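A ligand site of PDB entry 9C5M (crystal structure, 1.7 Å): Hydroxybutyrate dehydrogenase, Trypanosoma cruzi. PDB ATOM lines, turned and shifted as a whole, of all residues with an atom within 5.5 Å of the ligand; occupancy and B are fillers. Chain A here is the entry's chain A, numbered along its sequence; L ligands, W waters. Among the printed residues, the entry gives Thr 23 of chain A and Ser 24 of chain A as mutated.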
ATOM      1  N   THR A  20       4.855  14.944  18.293  1.00  0.00           N
ATOM      2  CA  THR A  20       3.936  14.058  17.598  1.00  0.00           C
ATOM      3  C   THR A  20       4.308  12.621  17.924  1.00  0.00           C
ATOM      4  O   THR A  20       5.477  12.305  18.143  1.00  0.00           O
ATOM      5  CB  THR A  20       3.965  14.315  16.088  1.00  0.00           C
ATOM      6  OG1 THR A  20       5.215  13.921  15.539  1.00  0.00           O
ATOM      7  CG2 THR A  20       3.702  15.808  15.799  1.00  0.00           C
ATOM      8  N   GLY A  21       3.305  11.762  18.056  1.00  0.00           N
ATOM      9  CA  GLY A  21       3.553  10.365  18.367  1.00  0.00           C
ATOM     10  C   GLY A  21       4.273  10.152  19.693  1.00  0.00           C
ATOM     11  O   GLY A  21       5.234   9.385  19.768  1.00  0.00           O
ATOM     12  N   SER A  22       3.792  10.818  20.738  1.00  0.00           N
ATOM     13  CA  SER A  22       4.438  10.797  22.051  1.00  0.00           C
ATOM     14  C   SER A  22       3.669   9.972  23.068  1.00  0.00           C
ATOM     15  O   SER A  22       3.878  10.124  24.277  1.00  0.00           O
ATOM     16  CB  SER A  22       4.640  12.228  22.565  1.00  0.00           C
ATOM     17  OG  SER A  22       3.460  13.002  22.425  1.00  0.00           O
ATOM     18  N   THR A  23       2.797   9.076  22.606  1.00  0.00           N
ATOM     19  CA  THR A  23       2.092   8.138  23.487  1.00  0.00           C
ATOM     20  C   THR A  23       2.853   6.834  23.667  1.00  0.00           C
ATOM     21  O   THR A  23       2.408   5.961  24.427  1.00  0.00           O
ATOM     22  CB  THR A  23       0.693   7.825  22.943  1.00  0.00           C
ATOM     23  OG1 THR A  23       0.816   7.276  21.616  1.00  0.00           O
ATOM     24  CG2 THR A  23      -0.189   9.070  22.937  1.00  0.00           C
ATOM     25  N   SER A  24       3.971   6.665  22.969  1.00  0.00           N
ATOM     26  CA  SER A  24       4.732   5.425  22.972  1.00  0.00           C
ATOM     27  C   SER A  24       6.197   5.748  22.703  1.00  0.00           C
ATOM     28  O   SER A  24       6.533   6.777  22.116  1.00  0.00           O
ATOM     29  CB  SER A  24       4.196   4.444  21.912  1.00  0.00           C
ATOM     30  OG  SER A  24       4.899   3.217  21.901  1.00  0.00           O
ATOM     31  N   GLY A  25       7.054   4.842  23.161  1.00  0.00           N
ATOM     32  CA  GLY A  25       8.418   4.762  22.678  1.00  0.00           C
ATOM     33  C   GLY A  25       9.219   6.050  22.762  1.00  0.00           C
ATOM     34  O   GLY A  25       9.252   6.748  23.801  1.00  0.00           O
ATOM     35  N   ILE A  26       9.924   6.347  21.660  1.00  0.00           N
ATOM     36  CA  ILE A  26      10.848   7.485  21.626  1.00  0.00           C
ATOM     37  C   ILE A  26      10.108   8.790  21.879  1.00  0.00           C
ATOM     38  O   ILE A  26      10.610   9.666  22.601  1.00  0.00           O
ATOM     39  CB  ILE A  26      11.606   7.506  20.293  1.00  0.00           C
ATOM     40  CG1 ILE A  26      12.623   6.366  20.273  1.00  0.00           C
ATOM     41  CG2 ILE A  26      12.286   8.866  20.050  1.00  0.00           C
ATOM     42  CD1 ILE A  26      13.238   6.105  18.927  1.00  0.00           C
ATOM     43  N   GLY A  27       8.937   8.975  21.276  1.00  0.00           N
ATOM     44  CA  GLY A  27       8.212  10.215  21.474  1.00  0.00           C
ATOM     45  C   GLY A  27       7.864  10.464  22.920  1.00  0.00           C
ATOM     46  O   GLY A  27       7.957  11.591  23.420  1.00  0.00           O
ATOM     47  N   ASN A  44       0.556  13.590  21.800  1.00  0.00           N
ATOM     48  CA  ASN A  44      -0.227  13.268  20.624  1.00  0.00           C
ATOM     49  C   ASN A  44      -0.056  11.795  20.280  1.00  0.00           C
ATOM     50  O   ASN A  44       1.044  11.250  20.358  1.00  0.00           O
ATOM     51  CB  ASN A  44       0.219  14.138  19.430  1.00  0.00           C
ATOM     52  CG  ASN A  44      -0.156  13.537  18.096  1.00  0.00           C
ATOM     53  OD1 ASN A  44       0.678  12.962  17.399  1.00  0.00           O
ATOM     54  ND2 ASN A  44      -1.426  13.669  17.733  1.00  0.00           N
ATOM     55  N   GLY A  45      -1.167  11.178  19.873  1.00  0.00           N
ATOM     56  CA  GLY A  45      -1.124   9.840  19.319  1.00  0.00           C
ATOM     57  C   GLY A  45      -2.151   9.720  18.204  1.00  0.00           C
ATOM     58  O   GLY A  45      -2.983  10.609  18.009  1.00  0.00           O
ATOM     59  N   ARG A  46      -2.070   8.600  17.485  1.00  0.00           N
ATOM     60  CA  ARG A  46      -2.917   8.407  16.315  1.00  0.00           C
ATOM     61  C   ARG A  46      -4.396   8.495  16.671  1.00  0.00           C
ATOM     62  O   ARG A  46      -5.174   9.143  15.954  1.00  0.00           O
ATOM     63  CB  ARG A  46      -2.584   7.049  15.681  1.00  0.00           C
ATOM     64  CG  ARG A  46      -3.514   6.575  14.588  1.00  0.00           C
ATOM     65  CD  ARG A  46      -3.648   7.584  13.460  1.00  0.00           C
ATOM     66  NE  ARG A  46      -4.582   7.111  12.440  1.00  0.00           N
ATOM     67  CZ  ARG A  46      -5.891   7.336  12.467  1.00  0.00           C
ATOM     68  NH1 ARG A  46      -6.460   8.023  13.446  1.00  0.00           N
ATOM     69  NH2 ARG A  46      -6.648   6.867  11.473  1.00  0.00           N
ATOM     70  N   ALA A  71      -4.652  13.011  17.040  1.00  0.00           N
ATOM     71  CA  ALA A  71      -4.689  13.563  15.701  1.00  0.00           C
ATOM     72  C   ALA A  71      -3.872  12.662  14.779  1.00  0.00           C
ATOM     73  O   ALA A  71      -2.757  12.274  15.137  1.00  0.00           O
ATOM     74  CB  ALA A  71      -4.146  15.000  15.688  1.00  0.00           C
ATOM     75  N   ASN A  72      -4.448  12.315  13.634  1.00  0.00           N
ATOM     76  CA  ASN A  72      -3.757  11.550  12.597  1.00  0.00           C
ATOM     77  C   ASN A  72      -2.874  12.501  11.809  1.00  0.00           C
ATOM     78  O   ASN A  72      -3.366  13.366  11.084  1.00  0.00           O
ATOM     79  CB  ASN A  72      -4.797  10.870  11.716  1.00  0.00           C
ATOM     80  CG  ASN A  72      -4.198  10.153  10.535  1.00  0.00           C
ATOM     81  OD1 ASN A  72      -2.974  10.022  10.429  1.00  0.00           O
ATOM     82  ND2 ASN A  72      -5.047   9.678   9.640  1.00  0.00           N
ATOM     83  N   MET A  73      -1.550  12.367  11.973  1.00  0.00           N
ATOM     84  CA  MET A  73      -0.604  13.286  11.345  1.00  0.00           C
ATOM     85  C   MET A  73      -0.542  13.142   9.835  1.00  0.00           C
ATOM     86  O   MET A  73       0.043  13.996   9.170  1.00  0.00           O
ATOM     87  CB  MET A  73       0.777  13.090  11.945  1.00  0.00           C
ATOM     88  CG  MET A  73       0.868  13.551  13.393  1.00  0.00           C
ATOM     89  SD  MET A  73       0.622  15.329  13.612  1.00  0.00           S
ATOM     90  CE  MET A  73      -1.125  15.472  14.021  1.00  0.00           C
ATOM     91  N   LYS A  74      -1.119  12.087   9.279  1.00  0.00           N
ATOM     92  CA  LYS A  74      -1.195  11.965   7.830  1.00  0.00           C
ATOM     93  C   LYS A  74      -2.271  12.861   7.209  1.00  0.00           C
ATOM     94  O   LYS A  74      -2.331  12.965   5.982  1.00  0.00           O
ATOM     95  CB  LYS A  74      -1.461  10.507   7.451  1.00  0.00           C
ATOM     96  CG  LYS A  74      -0.300   9.570   7.788  1.00  0.00           C
ATOM     97  CD  LYS A  74      -0.612   8.106   7.455  1.00  0.00           C
ATOM     98  CE  LYS A  74      -1.751   7.561   8.287  1.00  0.00           C
ATOM     99  NZ  LYS A  74      -1.960   6.110   8.079  1.00  0.00           N
ATOM    100  N   ASN A  99       8.014  13.407  15.290  1.00  0.00           N
ATOM    101  CA  ASN A  99       8.484  12.117  15.747  1.00  0.00           C
ATOM    102  C   ASN A  99       7.624  10.945  15.300  1.00  0.00           C
ATOM    103  O   ASN A  99       8.135   9.837  15.133  1.00  0.00           O
ATOM    104  CB  ASN A  99       8.562  12.092  17.283  1.00  0.00           C
ATOM    105  CG  ASN A  99       8.713  10.691  17.825  1.00  0.00           C
ATOM    106  OD1 ASN A  99       9.805  10.135  17.863  1.00  0.00           O
ATOM    107  ND2 ASN A  99       7.588  10.110  18.244  1.00  0.00           N
ATOM    108  N   ALA A 100       6.322  11.161  15.115  1.00  0.00           N
ATOM    109  CA  ALA A 100       5.433  10.066  14.765  1.00  0.00           C
ATOM    110  C   ALA A 100       5.943   9.371  13.518  1.00  0.00           C
ATOM    111  O   ALA A 100       6.286  10.020  12.521  1.00  0.00           O
ATOM    112  CB  ALA A 100       4.008  10.577  14.551  1.00  0.00           C
ATOM    113  N   GLY A 101       5.992   8.033  13.569  1.00  0.00           N
ATOM    114  CA  GLY A 101       6.521   7.251  12.464  1.00  0.00           C
ATOM    115  C   GLY A 101       6.126   5.803  12.553  1.00  0.00           C
ATOM    116  O   GLY A 101       5.777   5.291  13.616  1.00  0.00           O
ATOM    117  N   ILE A 102       6.190   5.137  11.396  1.00  0.00           N
ATOM    118  CA  ILE A 102       5.868   3.723  11.272  1.00  0.00           C
ATOM    119  C   ILE A 102       6.927   3.032  10.424  1.00  0.00           C
ATOM    120  O   ILE A 102       7.672   3.664   9.673  1.00  0.00           O
ATOM    121  CB  ILE A 102       4.482   3.477  10.657  1.00  0.00           C
ATOM    122  CG1 ILE A 102       4.372   4.180   9.309  1.00  0.00           C
ATOM    123  CG2 ILE A 102       3.375   3.941  11.592  1.00  0.00           C
ATOM    124  CD1 ILE A 102       3.173   3.779   8.535  1.00  0.00           C
ATOM    125  N   LEU A 122       3.597   9.679   6.439  1.00  0.00           N
ATOM    126  CA  LEU A 122       3.810   9.954   7.854  1.00  0.00           C
ATOM    127  C   LEU A 122       5.250  10.338   8.153  1.00  0.00           C
ATOM    128  O   LEU A 122       5.515  11.308   8.874  1.00  0.00           O
ATOM    129  CB  LEU A 122       3.405   8.754   8.698  1.00  0.00           C
ATOM    130  CG  LEU A 122       3.600   8.914  10.205  1.00  0.00           C
ATOM    131  CD1 LEU A 122       2.699  10.001  10.780  1.00  0.00           C
ATOM    132  CD2 LEU A 122       3.333   7.613  10.920  1.00  0.00           C
ATOM    133  N   ASN A 123       6.206   9.545   7.663  1.00  0.00           N
ATOM    134  CA  ASN A 123       7.577   9.710   8.117  1.00  0.00           C
ATOM    135  C   ASN A 123       8.279  10.882   7.453  1.00  0.00           C
ATOM    136  O   ASN A 123       9.370  11.263   7.901  1.00  0.00           O
ATOM    137  CB  ASN A 123       8.385   8.430   7.863  1.00  0.00           C
ATOM    138  CG  ASN A 123       7.904   7.251   8.689  1.00  0.00           C
ATOM    139  OD1 ASN A 123       6.778   7.219   9.185  1.00  0.00           O
ATOM    140  ND2 ASN A 123       8.770   6.248   8.836  1.00  0.00           N
ATOM    141  N   ILE A 149      12.824  13.642  14.120  1.00  0.00           N
ATOM    142  CA  ILE A 149      13.336  12.346  14.529  1.00  0.00           C
ATOM    143  C   ILE A 149      13.459  11.516  13.258  1.00  0.00           C
ATOM    144  O   ILE A 149      12.479  10.979  12.734  1.00  0.00           O
ATOM    145  CB  ILE A 149      12.452  11.673  15.577  1.00  0.00           C
ATOM    146  CG1 ILE A 149      12.240  12.633  16.757  1.00  0.00           C
ATOM    147  CG2 ILE A 149      13.123  10.371  16.020  1.00  0.00           C
ATOM    148  CD1 ILE A 149      13.523  13.178  17.363  1.00  0.00           C
ATOM    149  N   ALA A 150      14.682  11.456  12.740  1.00  0.00           N
ATOM    150  CA  ALA A 150      15.099  10.660  11.597  1.00  0.00           C
ATOM    151  C   ALA A 150      15.508   9.300  12.132  1.00  0.00           C
ATOM    152  O   ALA A 150      14.732   8.652  12.837  1.00  0.00           O
ATOM    153  CB  ALA A 150      16.204  11.343  10.808  1.00  0.00           C
ATOM    154  N   SER A 151      16.588   8.765  11.588  1.00  0.00           N
ATOM    155  CA  SER A 151      17.110   7.455  11.968  1.00  0.00           C
ATOM    156  C   SER A 151      18.493   7.315  11.366  1.00  0.00           C
ATOM    157  O   SER A 151      18.820   8.022  10.416  1.00  0.00           O
ATOM    158  CB  SER A 151      16.196   6.352  11.456  1.00  0.00           C
ATOM    159  OG  SER A 151      16.809   5.098  11.594  1.00  0.00           O
ATOM    160  N   VAL A 152      19.270   6.360  11.878  1.00  0.00           N
ATOM    161  CA  VAL A 152      20.449   5.898  11.140  1.00  0.00           C
ATOM    162  C   VAL A 152      20.037   5.512   9.725  1.00  0.00           C
ATOM    163  O   VAL A 152      20.844   5.596   8.780  1.00  0.00           O
ATOM    164  CB  VAL A 152      21.145   4.715  11.839  1.00  0.00           C
ATOM    165  CG1 VAL A 152      21.773   5.133  13.161  1.00  0.00           C
ATOM    166  CG2 VAL A 152      20.173   3.552  12.041  1.00  0.00           C
ATOM    167  N   TYR A 164      11.128   3.146   4.288  1.00  0.00           N
ATOM    168  CA  TYR A 164      11.557   3.813   5.511  1.00  0.00           C
ATOM    169  C   TYR A 164      12.888   4.523   5.310  1.00  0.00           C
ATOM    170  O   TYR A 164      13.034   5.685   5.696  1.00  0.00           O
ATOM    171  CB  TYR A 164      11.619   2.761   6.615  1.00  0.00           C
ATOM    172  CG  TYR A 164      11.928   3.227   8.011  1.00  0.00           C
ATOM    173  CD1 TYR A 164      13.244   3.342   8.445  1.00  0.00           C
ATOM    174  CD2 TYR A 164      10.910   3.469   8.929  1.00  0.00           C
ATOM    175  CE1 TYR A 164      13.528   3.720   9.758  1.00  0.00           C
ATOM    176  CE2 TYR A 164      11.187   3.847  10.219  1.00  0.00           C
ATOM    177  CZ  TYR A 164      12.490   3.971  10.635  1.00  0.00           C
ATOM    178  OH  TYR A 164      12.720   4.356  11.949  1.00  0.00           O
ATOM    179  N   LYS A 168      13.308   8.540   5.626  1.00  0.00           N
ATOM    180  CA  LYS A 168      14.205   9.096   6.631  1.00  0.00           C
ATOM    181  C   LYS A 168      15.335   9.893   5.981  1.00  0.00           C
ATOM    182  O   LYS A 168      15.731  10.969   6.483  1.00  0.00           O
ATOM    183  CB  LYS A 168      14.769   7.976   7.509  1.00  0.00           C
ATOM    184  CG  LYS A 168      13.727   7.310   8.412  1.00  0.00           C
ATOM    185  CD  LYS A 168      13.079   8.296   9.368  1.00  0.00           C
ATOM    186  CE  LYS A 168      12.275   7.573  10.453  1.00  0.00           C
ATOM    187  NZ  LYS A 168      11.569   8.501  11.394  1.00  0.00           N
ATOM    188  N   CYS A 193      19.217  11.136  14.836  1.00  0.00           N
ATOM    189  CA  CYS A 193      19.244   9.845  14.143  1.00  0.00           C
ATOM    190  C   CYS A 193      19.553   8.743  15.145  1.00  0.00           C
ATOM    191  O   CYS A 193      20.731   8.395  15.348  1.00  0.00           O
ATOM    192  CB  CYS A 193      20.276   9.844  13.013  1.00  0.00           C
ATOM    193  SG  CYS A 193      19.911  11.102  11.778  1.00  0.00           S
ATOM    194  N   PRO A 194      18.551   8.161  15.781  1.00  0.00           N
ATOM    195  CA  PRO A 194      18.811   7.010  16.640  1.00  0.00           C
ATOM    196  C   PRO A 194      19.112   5.750  15.847  1.00  0.00           C
ATOM    197  O   PRO A 194      18.602   5.556  14.737  1.00  0.00           O
ATOM    198  CB  PRO A 194      17.509   6.841  17.442  1.00  0.00           C
ATOM    199  CG  PRO A 194      16.667   8.060  17.134  1.00  0.00           C
ATOM    200  CD  PRO A 194      17.122   8.523  15.778  1.00  0.00           C
ATOM    201  N   GLY A 195      19.928   4.892  16.446  1.00  0.00           N
ATOM    202  CA  GLY A 195      19.987   3.492  16.102  1.00  0.00           C
ATOM    203  C   GLY A 195      18.865   2.763  16.815  1.00  0.00           C
ATOM    204  O   GLY A 195      17.859   3.363  17.210  1.00  0.00           O
ATOM    205  N   TYR A 196      19.044   1.464  17.031  1.00  0.00           N
ATOM    206  CA  TYR A 196      17.956   0.658  17.573  1.00  0.00           C
ATOM    207  C   TYR A 196      17.629   1.042  19.010  1.00  0.00           C
ATOM    208  O   TYR A 196      18.514   1.108  19.875  1.00  0.00           O
ATOM    209  CB  TYR A 196      18.317  -0.824  17.530  1.00  0.00           C
ATOM    210  CG  TYR A 196      18.256  -1.491  16.169  1.00  0.00           C
ATOM    211  CD1 TYR A 196      17.319  -1.114  15.217  1.00  0.00           C
ATOM    212  CD2 TYR A 196      19.129  -2.518  15.859  1.00  0.00           C
ATOM    213  CE1 TYR A 196      17.267  -1.756  13.972  1.00  0.00           C
ATOM    214  CE2 TYR A 196      19.092  -3.165  14.640  1.00  0.00           C
ATOM    215  CZ  TYR A 196      18.165  -2.768  13.685  1.00  0.00           C
ATOM    216  OH  TYR A 196      18.123  -3.422  12.471  1.00  0.00           O
ATOM    217  N   VAL A 197      16.338   1.245  19.269  1.00  0.00           N
ATOM    218  CA  VAL A 197      15.750   1.542  20.574  1.00  0.00           C
ATOM    219  C   VAL A 197      14.658   0.519  20.804  1.00  0.00           C
ATOM    220  O   VAL A 197      13.885   0.213  19.883  1.00  0.00           O
ATOM    221  CB  VAL A 197      15.183   2.972  20.615  1.00  0.00           C
ATOM    222  CG1 VAL A 197      14.605   3.279  21.998  1.00  0.00           C
ATOM    223  CG2 VAL A 197      16.244   3.994  20.208  1.00  0.00           C
ATOM    224  N   TYR A 198      14.570  -0.021  22.015  1.00  0.00           N
ATOM    225  CA  TYR A 198      13.622  -1.117  22.253  1.00  0.00           C
ATOM    226  C   TYR A 198      12.240  -0.527  22.538  1.00  0.00           C
ATOM    227  O   TYR A 198      11.792  -0.409  23.684  1.00  0.00           O
ATOM    228  CB  TYR A 198      14.087  -2.019  23.394  1.00  0.00           C
ATOM    229  CG  TYR A 198      13.399  -3.372  23.377  1.00  0.00           C
ATOM    230  CD1 TYR A 198      13.683  -4.304  22.389  1.00  0.00           C
ATOM    231  CD2 TYR A 198      12.466  -3.712  24.340  1.00  0.00           C
ATOM    232  CE1 TYR A 198      13.073  -5.546  22.362  1.00  0.00           C
ATOM    233  CE2 TYR A 198      11.838  -4.958  24.330  1.00  0.00           C
ATOM    234  CZ  TYR A 198      12.150  -5.867  23.322  1.00  0.00           C
ATOM    235  OH  TYR A 198      11.551  -7.111  23.284  1.00  0.00           O
ATOM    236  N   THR A 199      11.554  -0.180  21.458  1.00  0.00           N
ATOM    237  CA  THR A 199      10.182   0.266  21.428  1.00  0.00           C
ATOM    238  C   THR A 199       9.292  -0.781  20.766  1.00  0.00           C
ATOM    239  O   THR A 199       9.795  -1.728  20.152  1.00  0.00           O
ATOM    240  CB  THR A 199      10.082   1.558  20.614  1.00  0.00           C
ATOM    241  OG1 THR A 199      10.281   1.197  19.248  1.00  0.00           O
ATOM    242  CG2 THR A 199      11.143   2.582  21.054  1.00  0.00           C
ATOM    243  N   PRO A 200       7.971  -0.600  20.800  1.00  0.00           N
ATOM    244  CA  PRO A 200       7.101  -1.525  20.055  1.00  0.00           C
ATOM    245  C   PRO A 200       7.446  -1.637  18.565  1.00  0.00           C
ATOM    246  O   PRO A 200       7.319  -2.725  17.994  1.00  0.00           O
ATOM    247  CB  PRO A 200       5.696  -0.942  20.274  1.00  0.00           C
ATOM    248  CG  PRO A 200       5.792  -0.322  21.638  1.00  0.00           C
ATOM    249  CD  PRO A 200       7.183   0.279  21.699  1.00  0.00           C
ATOM    250  N   LEU A 201       7.891  -0.536  17.942  1.00  0.00           N
ATOM    251  CA  LEU A 201       8.240  -0.580  16.528  1.00  0.00           C
ATOM    252  C   LEU A 201       9.370  -1.570  16.261  1.00  0.00           C
ATOM    253  O   LEU A 201       9.375  -2.237  15.221  1.00  0.00           O
ATOM    254  CB  LEU A 201       8.619   0.823  16.047  1.00  0.00           C
ATOM    255  CG  LEU A 201       9.111   1.021  14.611  1.00  0.00           C
ATOM    256  CD1 LEU A 201       8.770   2.443  14.159  1.00  0.00           C
ATOM    257  CD2 LEU A 201      10.612   0.765  14.462  1.00  0.00           C
ATOM    258  N   VAL A 202      10.311  -1.691  17.186  1.00  0.00           N
ATOM    259  CA  VAL A 202      11.404  -2.663  17.081  1.00  0.00           C
ATOM    260  C   VAL A 202      11.008  -4.016  17.651  1.00  0.00           C
ATOM    261  O   VAL A 202      11.399  -5.062  17.127  1.00  0.00           O
ATOM    262  CB  VAL A 202      12.675  -2.107  17.766  1.00  0.00           C
ATOM    263  CG1 VAL A 202      13.646  -3.244  18.125  1.00  0.00           C
ATOM    264  CG2 VAL A 202      13.362  -1.071  16.869  1.00  0.00           C
HETATM  265  P1  LIG L   1       6.365   3.489  18.503  1.00  0.00           P
HETATM  266  O1  LIG L   1       6.804   3.063  19.773  1.00  0.00           O
HETATM  267  O2  LIG L   1       5.612   2.656  17.682  1.00  0.00           O
HETATM  268  O3  LIG L   1       5.681   4.862  18.595  1.00  0.00           O
HETATM  269  C1  LIG L   1       4.951   5.435  17.536  1.00  0.00           C
HETATM  270  C2  LIG L   1       4.199   6.676  17.918  1.00  0.00           C
HETATM  271  O4  LIG L   1       3.687   7.368  16.792  1.00  0.00           O
HETATM  272  C3  LIG L   1       2.977   6.349  18.782  1.00  0.00           C
HETATM  273  O5  LIG L   1       2.718   7.371  19.744  1.00  0.00           O
HETATM  274  C4  LIG L   1       1.832   6.329  17.758  1.00  0.00           C
HETATM  275  O6  LIG L   1       0.548   6.502  18.339  1.00  0.00           O
HETATM  276  C5  LIG L   1       2.270   7.480  16.858  1.00  0.00           C
HETATM  277  N1  LIG L   1       1.645   7.424  15.535  1.00  0.00           N
HETATM  278  C6  LIG L   1       1.705   6.458  14.630  1.00  0.00           C
HETATM  279  N2  LIG L   1       1.020   6.777  13.532  1.00  0.00           N
HETATM  280  C7  LIG L   1       0.543   7.986  13.712  1.00  0.00           C
HETATM  281  C8  LIG L   1      -0.256   8.946  12.944  1.00  0.00           C
HETATM  282  N3  LIG L   1      -0.684   8.663  11.728  1.00  0.00           N
HETATM  283  N4  LIG L   1      -0.561  10.095  13.510  1.00  0.00           N
HETATM  284  C9  LIG L   1      -0.133  10.397  14.713  1.00  0.00           C
HETATM  285  N5  LIG L   1       0.584   9.581  15.453  1.00  0.00           N
HETATM  286  C10 LIG L   1       0.973   8.406  15.017  1.00  0.00           C
HETATM  287  O7  LIG L   1       7.693   3.760  17.653  1.00  0.00           O
HETATM  288  P2  LIG L   1       9.040   4.456  18.029  1.00  0.00           P
HETATM  289  O8  LIG L   1      10.091   3.585  17.873  1.00  0.00           O
HETATM  290  O9  LIG L   1       9.039   5.195  19.263  1.00  0.00           O
HETATM  291  O10 LIG L   1       9.166   5.533  16.839  1.00  0.00           O
HETATM  292  C11 LIG L   1       9.187   6.899  17.053  1.00  0.00           C
HETATM  293  C12 LIG L   1      10.040   7.503  15.945  1.00  0.00           C
HETATM  294  O11 LIG L   1      11.352   7.090  16.117  1.00  0.00           O
HETATM  295  C13 LIG L   1       9.661   7.034  14.558  1.00  0.00           C
HETATM  296  O12 LIG L   1       9.748   8.149  13.686  1.00  0.00           O
HETATM  297  C14 LIG L   1      10.738   6.046  14.175  1.00  0.00           C
HETATM  298  O13 LIG L   1      10.987   6.003  12.807  1.00  0.00           O
HETATM  299  C15 LIG L   1      11.911   6.632  14.911  1.00  0.00           C
HETATM  300  N6  LIG L   1      12.993   5.731  15.172  1.00  0.00           N
HETATM  301  C16 LIG L   1      12.858   4.610  15.883  1.00  0.00           C
HETATM  302  C17 LIG L   1      13.900   3.789  16.143  1.00  0.00           C
HETATM  303  C18 LIG L   1      13.799   2.522  16.950  1.00  0.00           C
HETATM  304  O14 LIG L   1      14.709   1.847  16.992  1.00  0.00           O
HETATM  305  N7  LIG L   1      12.718   2.274  17.648  1.00  0.00           N
HETATM  306  C19 LIG L   1      15.257   4.105  15.623  1.00  0.00           C
HETATM  307  C20 LIG L   1      15.276   5.346  14.879  1.00  0.00           C
HETATM  308  C21 LIG L   1      14.153   6.081  14.699  1.00  0.00           C
HETATM  309  O   HOH W   1       2.979   2.093  18.338  1.00  0.00           O
HETATM  310  O   HOH W   2      -0.283   4.167  18.856  1.00  0.00           O
HETATM  311  O   HOH W   3       7.388   7.384  19.527  1.00  0.00           O
HETATM  312  O   HOH W   4      -0.191   5.772  11.035  1.00  0.00           O
HETATM  313  O   HOH W   5       4.945   2.977  14.762  1.00  0.00           O
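An oxygen (O5) of the ligand sits at hydrogen-bond distance from the backbone NH (N) of Thr 23, at 3.3 Å.
The backbone carbonyl oxygen (O) of Asn 99 is in hydrogen-bond range of an oxygen (O12) of the ligand, at 2.7 Å.
The side-chain hydroxyl (OH) of Tyr 164 lies within hydrogen-bond range of an oxygen (O13) of the ligand (2.5 Å).
The side-chain hydroxyl (OG1) of Thr 23 lies within hydrogen-bond range of an oxygen (O5) of the ligand (2.7 Å).
O of Gly 21 sits close to O5 of the ligand, 3.2 Å away.
A nitrogen (N4) of the ligand lies within hydrogen-bond range of the backbone NH (N) of Met 73 (2.9 Å).
An oxygen (O14) of the ligand sits at hydrogen-bond distance from the backbone NH (N) of Val 197.
The side-chain amide oxygen (OD1) of Asn 72 is in hydrogen-bond range of a nitrogen (N3) of the ligand (3.0 Å).
The backbone carbonyl oxygen of Val 197 sits at hydrogen-bond distance from a nitrogen (N7) of the ligand (3.3 Å).
The backbone NH (N) of Ile 26 sits at hydrogen-bond distance from an oxygen (O9) of the ligand (2.8 Å).
The backbone NH of Arg 46 is in hydrogen-bond range of an oxygen (O6) of the ligand (3.5 Å).
The side-chain hydroxyl of Ser 24 lies within hydrogen-bond range of an oxygen (O1) of the ligand (2.9 Å).
The side-chain hydroxyl of Thr 199 lies within hydrogen-bond range of an oxygen (O8) of the ligand (2.8 Å).
The side-chain amino group (NZ) of Lys 168 lies within hydrogen-bond range of an oxygen (O13) of the ligand (2.9 Å).
The backbone NH (N) of Leu 201 sits close to the side-chain hydroxyl (OG1) of Thr 199 (3.2 Å).
The backbone NH of Ala 71 is in hydrogen-bond range of the backbone carbonyl oxygen of Gly 45 (3.1 Å).
The backbone carbonyl oxygen (O) of Asn 44 sits at hydrogen-bond distance from the backbone NH (N) of Ser 22, 2.8 Å away.
The side-chain amide oxygen (OD1) of Asn 44 is in hydrogen-bond range of the backbone NH (N) of Gly 21 (3.0 Å).
The side-chain hydroxyl of Thr 20 lies within hydrogen-bond range of the backbone NH of Ala 100, at 3.0 Å.
The side-chain amino group of Lys 168 is in hydrogen-bond range of the backbone carbonyl oxygen of Ala 150.
O of Pro 194 lies within hydrogen-bond range of N of Val 152 (3.0 Å).
The side-chain sulfur (SG) of Cys 193 sits close to the backbone carbonyl oxygen (O) of Ser 151.
The backbone carbonyl oxygen (O) of Ala 71 lies close to a nitrogen (N4) of the ligand (3.5 Å).
Ser 22 touches the ligand.
Gly 25 touches the ligand.
Asn 44 touches the ligand (OD1 to C9, 3.8 Å).
CA of Gly 45 touches O6 of the ligand, at 3.9 Å.
Lys 74 touches the ligand.
CB of Ala 100 touches N5 of the ligand, at 3.7 Å.
Gly 101 touches the ligand.
Leu 122 touches the ligand.
CG2 of Ile 149 touches O11 of the ligand, at 3.7 Å.
Ala 150 touches the ligand.
OG of Ser 151 touches C20 of the ligand, at 3.6 Å.
O of Pro 194 touches C20 of the ligand, at 3.3 Å.
Gly 195 touches the ligand (O to C19, 3.1 Å).
Tyr 196 touches the ligand.
CD of Pro 200 touches O1 of the ligand (3.4 Å).
Leu 201 touches the ligand (CB to O7, 3.5 Å).
CG2 of Val 202 touches O14 of the ligand, at 3.2 Å.
Hydrophobic or aromatic side chains that line the ligand: Ile 26, Met 73, Ala 100, Leu 122, Ile 149, Tyr 164, Pro 194, Val 197, Pro 200, Leu 201 and Val 202.
Within 4 Å of the ligand: Gly 21, Ser 22, Thr 23, Ser 24, Gly 25, Ile 26, Asn 44, Gly 45, Arg 46, Ala 71, Asn 72, Met 73, Lys 74, Asn 99, Ala 100, Gly 101, Leu 122, Ile 149, Ala 150, Ser 151, Tyr 164, Lys 168, Pro 194, Gly 195, Tyr 196, Val 197, Thr 199, Pro 200, Leu 201 and Val 202.
Water W4 bridges N2 of the ligand and NZ of Lys 74.
Water W5 bridges the backbone carbonyl oxygen of Gly 101 (2.7 Å) and an oxygen (O2) of the ligand (3.0 Å).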
